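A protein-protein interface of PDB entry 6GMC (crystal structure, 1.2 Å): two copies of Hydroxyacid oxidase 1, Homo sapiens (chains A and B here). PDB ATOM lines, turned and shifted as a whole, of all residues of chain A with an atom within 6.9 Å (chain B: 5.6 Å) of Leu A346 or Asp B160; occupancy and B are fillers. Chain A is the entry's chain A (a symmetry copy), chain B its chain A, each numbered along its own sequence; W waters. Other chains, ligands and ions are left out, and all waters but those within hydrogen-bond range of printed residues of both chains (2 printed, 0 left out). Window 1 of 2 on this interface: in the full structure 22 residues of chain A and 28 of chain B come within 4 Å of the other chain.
OH of Tyr B163 lies within hydrogen-bond range of O of Val A57 (3.1 Å). The backbone carbonyl oxygen of Val B159 sits close to the side-chain sulfur of Met A53, at 3.4 Å.
N of Val B159 is in hydrogen-bond range of O of Lys B236 (2.9 Å). The side-chain carboxylate of Asp B160 is in hydrogen-bond range of the side-chain hydroxyl of Thr B161, at 2.8 Å. The side-chain amide nitrogen (NE2) of Gln B264 sits at hydrogen-bond distance from the backbone carbonyl oxygen (O) of Asp B160 (3.1 Å). The backbone carbonyl oxygen (O) of Tyr B163 sits at hydrogen-bond distance from the side-chain amide nitrogen (NE2) of Gln B264 (2.9 Å). The side-chain amide oxygen (OE1) of Gln B264 sits at hydrogen-bond distance from the backbone NH (N) of Gly B165 (2.9 Å).
Pro A51 touches Leu B265 (CB to CD2, 3.9 Å). Met A53 touches Asp B160. Val B159 touches Leu A54. Val A57 touches Pro B162 (CG2 to CB, 3.8 Å). CD1 of Leu A342 touches CB of Tyr B163, at 3.8 Å. Leu A342 touches Leu B164. O of Asp B160 touches CD2 of Leu A346, at 3.9 Å. Leu A346 touches Pro B162. Leu A346 touches Gln B264. N of Leu B265 touches CD1 of Leu A346 (3.8 Å).
Of the printed residues of chain B, Met A53 touches Val B159 (3.4 Å), Asp B160 (3.7 Å) and Gly B237 (3.3 Å). Of chain B, only Asp B160 (3.9 Å), Pro B162 (3.9 Å), Tyr B163 (3.4 Å), Gln B264 (3.6 Å) and Leu B265 (3.8 Å) come within 4 Å of Leu A346. Of the printed residues of chain A, Val B159 touches Met A53 (3.4 Å) and Leu A54 (3.9 Å). Asp B160 touches just these residues of chain A: Met A53 (3.7 Å) and Leu A346 (3.9 Å). Lys B236 touches none of the printed residues of chain A.
Along chain A the printed residues that touch a printed residue of chain B span positions 51 to 346. Of the 16 printed residues of chain B, 8 touch a printed residue of chain A. Printed residues of chain B that touch a printed residue of chain A: Val B159, Asp B160, Pro B162, Tyr B163, Leu B164, Gly B237, Gln B264 and Leu B265. Hydrophobic or aromatic side chains of chain B within 4 Å of the printed part of chain A: Val B159, Pro B162, Tyr B163 and Leu B265. Among the printed residues, 15 pairs touch across the chains.
No position is printed for both chains.
Water W2 lies within hydrogen-bond range of OG1 of Thr A60 (2.7 Å), OH of Tyr B163 (3.0 Å) and O of Val A57 (3.4 Å). Water W1 bridges O of Leu A346 (2.9 Å) and O of Asp B160 (2.9 Å).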
ATOM      1  N   PRO A  51      25.120 -27.065   4.675  1.00  0.00           N
ATOM      2  CA  PRO A  51      25.527 -25.808   5.290  1.00  0.00           C
ATOM      3  C   PRO A  51      26.298 -26.009   6.594  1.00  0.00           C
ATOM      4  O   PRO A  51      26.000 -26.904   7.374  1.00  0.00           O
ATOM      5  CB  PRO A  51      24.196 -25.117   5.597  1.00  0.00           C
ATOM      6  CG  PRO A  51      23.228 -26.255   5.774  1.00  0.00           C
ATOM      7  CD  PRO A  51      23.668 -27.261   4.731  1.00  0.00           C
ATOM      8  N   ARG A  52      27.297 -25.146   6.806  1.00  0.00           N
ATOM      9  CA  ARG A  52      28.017 -25.080   8.067  1.00  0.00           C
ATOM     10  C   ARG A  52      27.339 -24.057   8.973  1.00  0.00           C
ATOM     11  O   ARG A  52      27.011 -22.945   8.535  1.00  0.00           O
ATOM     12  CB  ARG A  52      29.467 -24.643   7.878  1.00  0.00           C
ATOM     13  CG  ARG A  52      30.332 -25.662   7.161  1.00  0.00           C
ATOM     14  CD  ARG A  52      31.757 -25.151   7.147  1.00  0.00           C
ATOM     15  NE  ARG A  52      32.676 -26.033   6.460  1.00  0.00           N
ATOM     16  CZ  ARG A  52      32.929 -26.000   5.158  1.00  0.00           C
ATOM     17  NH1 ARG A  52      33.858 -26.798   4.662  1.00  0.00           N
ATOM     18  NH2 ARG A  52      32.251 -25.191   4.360  1.00  0.00           N
ATOM     19  N   MET A  53      27.173 -24.443  10.241  1.00  0.00           N
ATOM     20  CA  MET A  53      26.574 -23.598  11.251  1.00  0.00           C
ATOM     21  C   MET A  53      27.653 -22.848  12.047  1.00  0.00           C
ATOM     22  O   MET A  53      28.814 -23.270  12.136  1.00  0.00           O
ATOM     23  CB  MET A  53      25.722 -24.446  12.203  1.00  0.00           C
ATOM     24  CG  MET A  53      24.677 -25.272  11.479  1.00  0.00           C
ATOM     25  SD  MET A  53      23.542 -24.242  10.542  1.00  0.00           S
ATOM     26  CE  MET A  53      23.043 -25.387   9.260  1.00  0.00           C
ATOM     27  N   LEU A  54      27.235 -21.732  12.655  1.00  0.00           N
ATOM     28  CA  LEU A  54      28.033 -20.997  13.647  1.00  0.00           C
ATOM     29  C   LEU A  54      29.355 -20.496  13.052  1.00  0.00           C
ATOM     30  O   LEU A  54      30.415 -20.569  13.723  1.00  0.00           O
ATOM     31  CB  LEU A  54      28.267 -21.914  14.854  1.00  0.00           C
ATOM     32  CG  LEU A  54      27.000 -22.352  15.577  1.00  0.00           C
ATOM     33  CD1 LEU A  54      27.295 -23.494  16.540  1.00  0.00           C
ATOM     34  CD2 LEU A  54      26.372 -21.184  16.311  1.00  0.00           C
ATOM     35  N   VAL A  57      28.414 -14.791  10.043  1.00  0.00           N
ATOM     36  CA  VAL A  57      28.007 -14.334   8.722  1.00  0.00           C
ATOM     37  C   VAL A  57      27.349 -12.949   8.836  1.00  0.00           C
ATOM     38  O   VAL A  57      26.484 -12.586   8.036  1.00  0.00           O
ATOM     39  CB  VAL A  57      27.103 -15.380   8.045  1.00  0.00           C
ATOM     40  CG1 VAL A  57      27.886 -16.636   7.701  1.00  0.00           C
ATOM     41  CG2 VAL A  57      25.892 -15.734   8.891  1.00  0.00           C
ATOM     42  N   THR A  60      28.563 -10.350   5.220  1.00  0.00           N
ATOM     43  CA  THR A  60      28.741 -11.120   4.004  1.00  0.00           C
ATOM     44  C   THR A  60      29.260 -10.215   2.885  1.00  0.00           C
ATOM     45  O   THR A  60      28.730  -9.114   2.662  1.00  0.00           O
ATOM     46  CB  THR A  60      27.432 -11.785   3.586  1.00  0.00           C
ATOM     47  OG1 THR A  60      26.473 -10.730   3.497  1.00  0.00           O
ATOM     48  CG2 THR A  60      26.998 -12.853   4.565  1.00  0.00           C
ATOM     49  N   LEU A 301      25.228 -20.292  -5.614  1.00  0.00           N
ATOM     50  CA  LEU A 301      26.051 -20.909  -4.578  1.00  0.00           C
ATOM     51  C   LEU A 301      26.549 -22.286  -5.024  1.00  0.00           C
ATOM     52  O   LEU A 301      27.716 -22.625  -4.826  1.00  0.00           O
ATOM     53  CB  LEU A 301      25.250 -21.002  -3.282  1.00  0.00           C
ATOM     54  CG  LEU A 301      26.002 -21.556  -2.072  1.00  0.00           C
ATOM     55  CD1 LEU A 301      27.191 -20.681  -1.721  1.00  0.00           C
ATOM     56  CD2 LEU A 301      25.068 -21.685  -0.881  1.00  0.00           C
ATOM     57  N   PHE A 340      21.368 -14.693  -3.174  1.00  0.00           N
ATOM     58  CA  PHE A 340      22.706 -15.260  -3.051  1.00  0.00           C
ATOM     59  C   PHE A 340      23.313 -14.912  -1.687  1.00  0.00           C
ATOM     60  O   PHE A 340      23.905 -15.769  -1.036  1.00  0.00           O
ATOM     61  CB  PHE A 340      23.581 -14.809  -4.222  1.00  0.00           C
ATOM     62  CG  PHE A 340      24.997 -15.316  -4.137  1.00  0.00           C
ATOM     63  CD1 PHE A 340      25.253 -16.679  -4.051  1.00  0.00           C
ATOM     64  CD2 PHE A 340      26.076 -14.445  -4.141  1.00  0.00           C
ATOM     65  CE1 PHE A 340      26.555 -17.150  -3.959  1.00  0.00           C
ATOM     66  CE2 PHE A 340      27.376 -14.920  -4.055  1.00  0.00           C
ATOM     67  CZ  PHE A 340      27.615 -16.272  -3.964  1.00  0.00           C
ATOM     68  N   ARG A 341      23.150 -13.657  -1.256  1.00  0.00           N
ATOM     69  CA  ARG A 341      23.631 -13.238   0.066  1.00  0.00           C
ATOM     70  C   ARG A 341      23.036 -14.137   1.156  1.00  0.00           C
ATOM     71  O   ARG A 341      23.747 -14.616   2.038  1.00  0.00           O
ATOM     72  CB  ARG A 341      23.274 -11.777   0.326  1.00  0.00           C
ATOM     73  CG  ARG A 341      23.902 -11.252   1.598  1.00  0.00           C
ATOM     74  CD  ARG A 341      23.620  -9.785   1.865  1.00  0.00           C
ATOM     75  NE  ARG A 341      23.974  -8.892   0.764  1.00  0.00           N
ATOM     76  CZ  ARG A 341      25.180  -8.363   0.555  1.00  0.00           C
ATOM     77  NH1 ARG A 341      26.207  -8.705   1.313  1.00  0.00           N
ATOM     78  NH2 ARG A 341      25.357  -7.487  -0.419  1.00  0.00           N
ATOM     79  N   LEU A 342      21.715 -14.355   1.099  1.00  0.00           N
ATOM     80  CA  LEU A 342      21.056 -15.168   2.116  1.00  0.00           C
ATOM     81  C   LEU A 342      21.568 -16.614   2.060  1.00  0.00           C
ATOM     82  O   LEU A 342      21.826 -17.219   3.099  1.00  0.00           O
ATOM     83  CB  LEU A 342      19.537 -15.104   1.959  1.00  0.00           C
ATOM     84  CG  LEU A 342      18.731 -15.893   2.994  1.00  0.00           C
ATOM     85  CD1 LEU A 342      18.981 -15.359   4.398  1.00  0.00           C
ATOM     86  CD2 LEU A 342      17.253 -15.849   2.664  1.00  0.00           C
ATOM     87  N   ALA A 343      21.715 -17.165   0.853  1.00  0.00           N
ATOM     88  CA  ALA A 343      22.192 -18.534   0.706  1.00  0.00           C
ATOM     89  C   ALA A 343      23.608 -18.671   1.284  1.00  0.00           C
ATOM     90  O   ALA A 343      23.927 -19.653   1.962  1.00  0.00           O
ATOM     91  CB  ALA A 343      22.136 -18.959  -0.739  1.00  0.00           C
ATOM     92  N   MET A 344      24.464 -17.693   0.991  1.00  0.00           N
ATOM     93  CA  MET A 344      25.808 -17.663   1.557  1.00  0.00           C
ATOM     94  C   MET A 344      25.731 -17.660   3.089  1.00  0.00           C
ATOM     95  O   MET A 344      26.392 -18.458   3.765  1.00  0.00           O
ATOM     96  CB  MET A 344      26.587 -16.426   1.101  1.00  0.00           C
ATOM     97  CG  MET A 344      27.215 -16.591  -0.251  1.00  0.00           C
ATOM     98  SD  MET A 344      28.092 -15.094  -0.758  1.00  0.00           S
ATOM     99  CE  MET A 344      29.417 -15.088   0.439  1.00  0.00           C
ATOM    100  N   ALA A 345      24.941 -16.747   3.640  1.00  0.00           N
ATOM    101  CA  ALA A 345      24.883 -16.602   5.092  1.00  0.00           C
ATOM    102  C   ALA A 345      24.356 -17.886   5.745  1.00  0.00           C
ATOM    103  O   ALA A 345      24.918 -18.357   6.742  1.00  0.00           O
ATOM    104  CB  ALA A 345      24.027 -15.420   5.457  1.00  0.00           C
ATOM    105  N   LEU A 346      23.277 -18.452   5.186  1.00  0.00           N
ATOM    106  CA  LEU A 346      22.685 -19.625   5.816  1.00  0.00           C
ATOM    107  C   LEU A 346      23.591 -20.854   5.679  1.00  0.00           C
ATOM    108  O   LEU A 346      23.422 -21.809   6.434  1.00  0.00           O
ATOM    109  CB  LEU A 346      21.306 -19.903   5.224  1.00  0.00           C
ATOM    110  CG  LEU A 346      20.247 -18.839   5.483  1.00  0.00           C
ATOM    111  CD1 LEU A 346      18.926 -19.296   4.889  1.00  0.00           C
ATOM    112  CD2 LEU A 346      20.109 -18.514   6.968  1.00  0.00           C
ATOM    113  N   SER A 347      24.542 -20.830   4.741  1.00  0.00           N
ATOM    114  CA  SER A 347      25.459 -21.963   4.562  1.00  0.00           C
ATOM    115  C   SER A 347      26.799 -21.736   5.271  1.00  0.00           C
ATOM    116  O   SER A 347      27.663 -22.607   5.202  1.00  0.00           O
ATOM    117  CB  SER A 347      25.661 -22.279   3.102  1.00  0.00           C
ATOM    118  OG  SER A 347      26.341 -21.227   2.427  1.00  0.00           O
ATOM    119  N   GLY A 348      26.956 -20.591   5.947  1.00  0.00           N
ATOM    120  CA  GLY A 348      28.179 -20.326   6.722  1.00  0.00           C
ATOM    121  C   GLY A 348      29.304 -19.674   5.942  1.00  0.00           C
ATOM    122  O   GLY A 348      30.429 -19.704   6.411  1.00  0.00           O
ATOM    123  N   CYS A 349      29.002 -19.031   4.813  1.00  0.00           N
ATOM    124  CA  CYS A 349      30.012 -18.442   3.949  1.00  0.00           C
ATOM    125  C   CYS A 349      29.991 -16.915   4.074  1.00  0.00           C
ATOM    126  O   CYS A 349      29.052 -16.272   3.647  1.00  0.00           O
ATOM    127  CB  CYS A 349      29.779 -18.811   2.494  1.00  0.00           C
ATOM    128  SG  CYS A 349      29.807 -20.593   2.190  1.00  0.00           S
ATOM    129  N   TYR B 132      17.306 -18.711  20.936  1.00  0.00           N
ATOM    130  CA  TYR B 132      18.206 -18.058  20.037  1.00  0.00           C
ATOM    131  C   TYR B 132      19.184 -17.204  20.831  1.00  0.00           C
ATOM    132  O   TYR B 132      18.802 -16.641  21.853  1.00  0.00           O
ATOM    133  CB  TYR B 132      17.455 -17.118  19.107  1.00  0.00           C
ATOM    134  CG  TYR B 132      16.683 -17.833  18.046  1.00  0.00           C
ATOM    135  CD1 TYR B 132      17.355 -18.521  17.054  1.00  0.00           C
ATOM    136  CD2 TYR B 132      15.305 -17.804  18.024  1.00  0.00           C
ATOM    137  CE1 TYR B 132      16.665 -19.181  16.059  1.00  0.00           C
ATOM    138  CE2 TYR B 132      14.596 -18.444  17.026  1.00  0.00           C
ATOM    139  CZ  TYR B 132      15.285 -19.132  16.042  1.00  0.00           C
ATOM    140  OH  TYR B 132      14.638 -19.776  15.041  1.00  0.00           O
ATOM    141  N   THR B 158      19.098 -22.971  18.753  1.00  0.00           N
ATOM    142  CA  THR B 158      18.920 -23.050  17.316  1.00  0.00           C
ATOM    143  C   THR B 158      20.082 -22.326  16.640  1.00  0.00           C
ATOM    144  O   THR B 158      20.345 -21.170  16.962  1.00  0.00           O
ATOM    145  CB  THR B 158      17.573 -22.470  16.897  1.00  0.00           C
ATOM    146  OG1 THR B 158      16.585 -23.231  17.588  1.00  0.00           O
ATOM    147  CG2 THR B 158      17.352 -22.556  15.405  1.00  0.00           C
ATOM    148  N   VAL B 159      20.752 -23.018  15.711  1.00  0.00           N
ATOM    149  CA  VAL B 159      21.985 -22.519  15.108  1.00  0.00           C
ATOM    150  C   VAL B 159      21.874 -22.310  13.597  1.00  0.00           C
ATOM    151  O   VAL B 159      22.882 -21.968  12.986  1.00  0.00           O
ATOM    152  CB  VAL B 159      23.176 -23.435  15.442  1.00  0.00           C
ATOM    153  CG1 VAL B 159      23.374 -23.533  16.941  1.00  0.00           C
ATOM    154  CG2 VAL B 159      23.046 -24.817  14.822  1.00  0.00           C
ATOM    155  N   ASP B 160      20.685 -22.491  13.011  1.00  0.00           N
ATOM    156  CA  ASP B 160      20.529 -22.440  11.554  1.00  0.00           C
ATOM    157  C   ASP B 160      19.811 -21.176  11.061  1.00  0.00           C
ATOM    158  O   ASP B 160      19.480 -21.093   9.875  1.00  0.00           O
ATOM    159  CB  ASP B 160      19.812 -23.700  11.077  1.00  0.00           C
ATOM    160  CG  ASP B 160      18.415 -23.925  11.637  1.00  0.00           C
ATOM    161  OD1 ASP B 160      17.863 -22.984  12.264  1.00  0.00           O
ATOM    162  OD2 ASP B 160      17.886 -25.050  11.434  1.00  0.00           O
ATOM    163  N   THR B 161      19.631 -20.185  11.944  1.00  0.00           N
ATOM    164  CA  THR B 161      18.805 -19.006  11.652  1.00  0.00           C
ATOM    165  C   THR B 161      19.572 -17.731  12.003  1.00  0.00           C
ATOM    166  O   THR B 161      19.067 -16.881  12.732  1.00  0.00           O
ATOM    167  CB  THR B 161      17.456 -19.101  12.382  1.00  0.00           C
ATOM    168  OG1 THR B 161      16.885 -20.377  12.103  1.00  0.00           O
ATOM    169  CG2 THR B 161      16.441 -18.059  11.969  1.00  0.00           C
ATOM    170  N   PRO B 162      20.777 -17.492  11.441  1.00  0.00           N
ATOM    171  CA  PRO B 162      21.440 -16.200  11.634  1.00  0.00           C
ATOM    172  C   PRO B 162      20.620 -15.076  10.989  1.00  0.00           C
ATOM    173  O   PRO B 162      20.686 -13.931  11.422  1.00  0.00           O
ATOM    174  CB  PRO B 162      22.801 -16.390  10.956  1.00  0.00           C
ATOM    175  CG  PRO B 162      22.542 -17.450   9.913  1.00  0.00           C
ATOM    176  CD  PRO B 162      21.560 -18.392  10.583  1.00  0.00           C
ATOM    177  N   TYR B 163      19.887 -15.446   9.937  1.00  0.00           N
ATOM    178  CA  TYR B 163      18.855 -14.652   9.282  1.00  0.00           C
ATOM    179  C   TYR B 163      17.668 -15.578   9.023  1.00  0.00           C
ATOM    180  O   TYR B 163      17.859 -16.793   8.936  1.00  0.00           O
ATOM    181  CB  TYR B 163      19.346 -14.084   7.948  1.00  0.00           C
ATOM    182  CG  TYR B 163      20.566 -13.212   8.085  1.00  0.00           C
ATOM    183  CD1 TYR B 163      20.467 -11.888   8.485  1.00  0.00           C
ATOM    184  CD2 TYR B 163      21.831 -13.708   7.833  1.00  0.00           C
ATOM    185  CE1 TYR B 163      21.586 -11.088   8.633  1.00  0.00           C
ATOM    186  CE2 TYR B 163      22.962 -12.918   7.967  1.00  0.00           C
ATOM    187  CZ  TYR B 163      22.842 -11.605   8.376  1.00  0.00           C
ATOM    188  OH  TYR B 163      23.964 -10.835   8.523  1.00  0.00           O
ATOM    189  N   LEU B 164      16.470 -15.018   8.835  1.00  0.00           N
ATOM    190  CA  LEU B 164      15.312 -15.859   8.496  1.00  0.00           C
ATOM    191  C   LEU B 164      15.378 -16.297   7.031  1.00  0.00           C
ATOM    192  O   LEU B 164      15.759 -15.537   6.148  1.00  0.00           O
ATOM    193  CB  LEU B 164      14.018 -15.090   8.763  1.00  0.00           C
ATOM    194  CG  LEU B 164      12.772 -15.965   8.901  1.00  0.00           C
ATOM    195  CD1 LEU B 164      12.796 -16.775  10.185  1.00  0.00           C
ATOM    196  CD2 LEU B 164      11.518 -15.109   8.862  1.00  0.00           C
ATOM    197  N   GLY B 165      14.963 -17.540   6.779  1.00  0.00           N
ATOM    198  CA  GLY B 165      14.760 -18.006   5.414  1.00  0.00           C
ATOM    199  C   GLY B 165      13.706 -17.180   4.699  1.00  0.00           C
ATOM    200  O   GLY B 165      12.902 -16.485   5.307  1.00  0.00           O
ATOM    201  N   LYS B 236      20.471 -27.398  17.779  1.00  0.00           N
ATOM    202  CA  LYS B 236      19.351 -27.637  16.891  1.00  0.00           C
ATOM    203  C   LYS B 236      19.638 -27.000  15.533  1.00  0.00           C
ATOM    204  O   LYS B 236      19.836 -25.784  15.427  1.00  0.00           O
ATOM    205  CB  LYS B 236      18.086 -27.047  17.506  1.00  0.00           C
ATOM    206  CG  LYS B 236      16.836 -27.097  16.640  1.00  0.00           C
ATOM    207  CD  LYS B 236      15.610 -26.641  17.407  1.00  0.00           C
ATOM    208  CE  LYS B 236      14.315 -26.740  16.624  1.00  0.00           C
ATOM    209  NZ  LYS B 236      14.225 -25.732  15.546  1.00  0.00           N
ATOM    210  N   GLY B 237      19.597 -27.832  14.490  1.00  0.00           N
ATOM    211  CA  GLY B 237      19.790 -27.362  13.111  1.00  0.00           C
ATOM    212  C   GLY B 237      21.075 -27.835  12.445  1.00  0.00           C
ATOM    213  O   GLY B 237      21.392 -27.386  11.353  1.00  0.00           O
ATOM    214  N   SER B 258      18.089 -31.268  12.037  1.00  0.00           N
ATOM    215  CA  SER B 258      16.964 -30.427  11.694  1.00  0.00           C
ATOM    216  C   SER B 258      17.379 -29.524  10.542  1.00  0.00           C
ATOM    217  O   SER B 258      18.485 -29.005  10.545  1.00  0.00           O
ATOM    218  CB  SER B 258      16.521 -29.593  12.889  1.00  0.00           C
ATOM    219  OG  SER B 258      15.448 -28.723  12.547  1.00  0.00           O
ATOM    220  N   ASN B 259      16.449 -29.341   9.599  1.00  0.00           N
ATOM    221  CA  ASN B 259      16.570 -28.292   8.594  1.00  0.00           C
ATOM    222  C   ASN B 259      15.500 -27.221   8.838  1.00  0.00           C
ATOM    223  O   ASN B 259      15.116 -26.493   7.923  1.00  0.00           O
ATOM    224  CB  ASN B 259      16.570 -28.860   7.173  1.00  0.00           C
ATOM    225  CG  ASN B 259      15.410 -29.782   6.877  1.00  0.00           C
ATOM    226  OD1 ASN B 259      14.305 -29.574   7.398  1.00  0.00           O
ATOM    227  ND2 ASN B 259      15.651 -30.792   6.040  1.00  0.00           N
ATOM    228  N   HIS B 260      15.070 -27.099  10.101  1.00  0.00           N
ATOM    229  CA  HIS B 260      14.138 -26.042  10.512  1.00  0.00           C
ATOM    230  C   HIS B 260      12.808 -26.205   9.760  1.00  0.00           C
ATOM    231  O   HIS B 260      12.207 -25.231   9.342  1.00  0.00           O
ATOM    232  CB  HIS B 260      14.756 -24.660  10.272  1.00  0.00           C
ATOM    233  CG  HIS B 260      14.307 -23.581  11.195  1.00  0.00           C
ATOM    234  ND1 HIS B 260      13.044 -22.994  11.258  1.00  0.00           N
ATOM    235  CD2 HIS B 260      15.067 -22.905  12.087  1.00  0.00           C
ATOM    236  CE1 HIS B 260      13.082 -22.011  12.177  1.00  0.00           C
ATOM    237  NE2 HIS B 260      14.299 -21.958  12.688  1.00  0.00           N
ATOM    238  N   GLN B 264      14.511 -22.689   6.165  1.00  0.00           N
ATOM    239  CA  GLN B 264      15.728 -21.876   6.198  1.00  0.00           C
ATOM    240  C   GLN B 264      16.413 -21.976   4.829  1.00  0.00           C
ATOM    241  O   GLN B 264      15.984 -21.290   3.919  1.00  0.00           O
ATOM    242  CB  GLN B 264      16.573 -22.258   7.413  1.00  0.00           C
ATOM    243  CG  GLN B 264      15.967 -21.741   8.710  1.00  0.00           C
ATOM    244  CD  GLN B 264      15.909 -20.232   8.723  1.00  0.00           C
ATOM    245  OE1 GLN B 264      14.833 -19.636   8.720  1.00  0.00           O
ATOM    246  NE2 GLN B 264      17.079 -19.601   8.671  1.00  0.00           N
ATOM    247  N   LEU B 265      17.481 -22.766   4.692  1.00  0.00           N
ATOM    248  CA  LEU B 265      18.151 -22.916   3.395  1.00  0.00           C
ATOM    249  C   LEU B 265      17.423 -24.007   2.610  1.00  0.00           C
ATOM    250  O   LEU B 265      17.342 -25.143   3.081  1.00  0.00           O
ATOM    251  CB  LEU B 265      19.619 -23.278   3.635  1.00  0.00           C
ATOM    252  CG  LEU B 265      20.499 -23.400   2.396  1.00  0.00           C
ATOM    253  CD1 LEU B 265      20.511 -22.121   1.560  1.00  0.00           C
ATOM    254  CD2 LEU B 265      21.908 -23.801   2.794  1.00  0.00           C
HETATM  255  O   HOH W   1      20.967 -22.555   7.800  1.00  0.00           O
HETATM  256  O   HOH W   2      25.139 -10.332   5.832  1.00  0.00           O
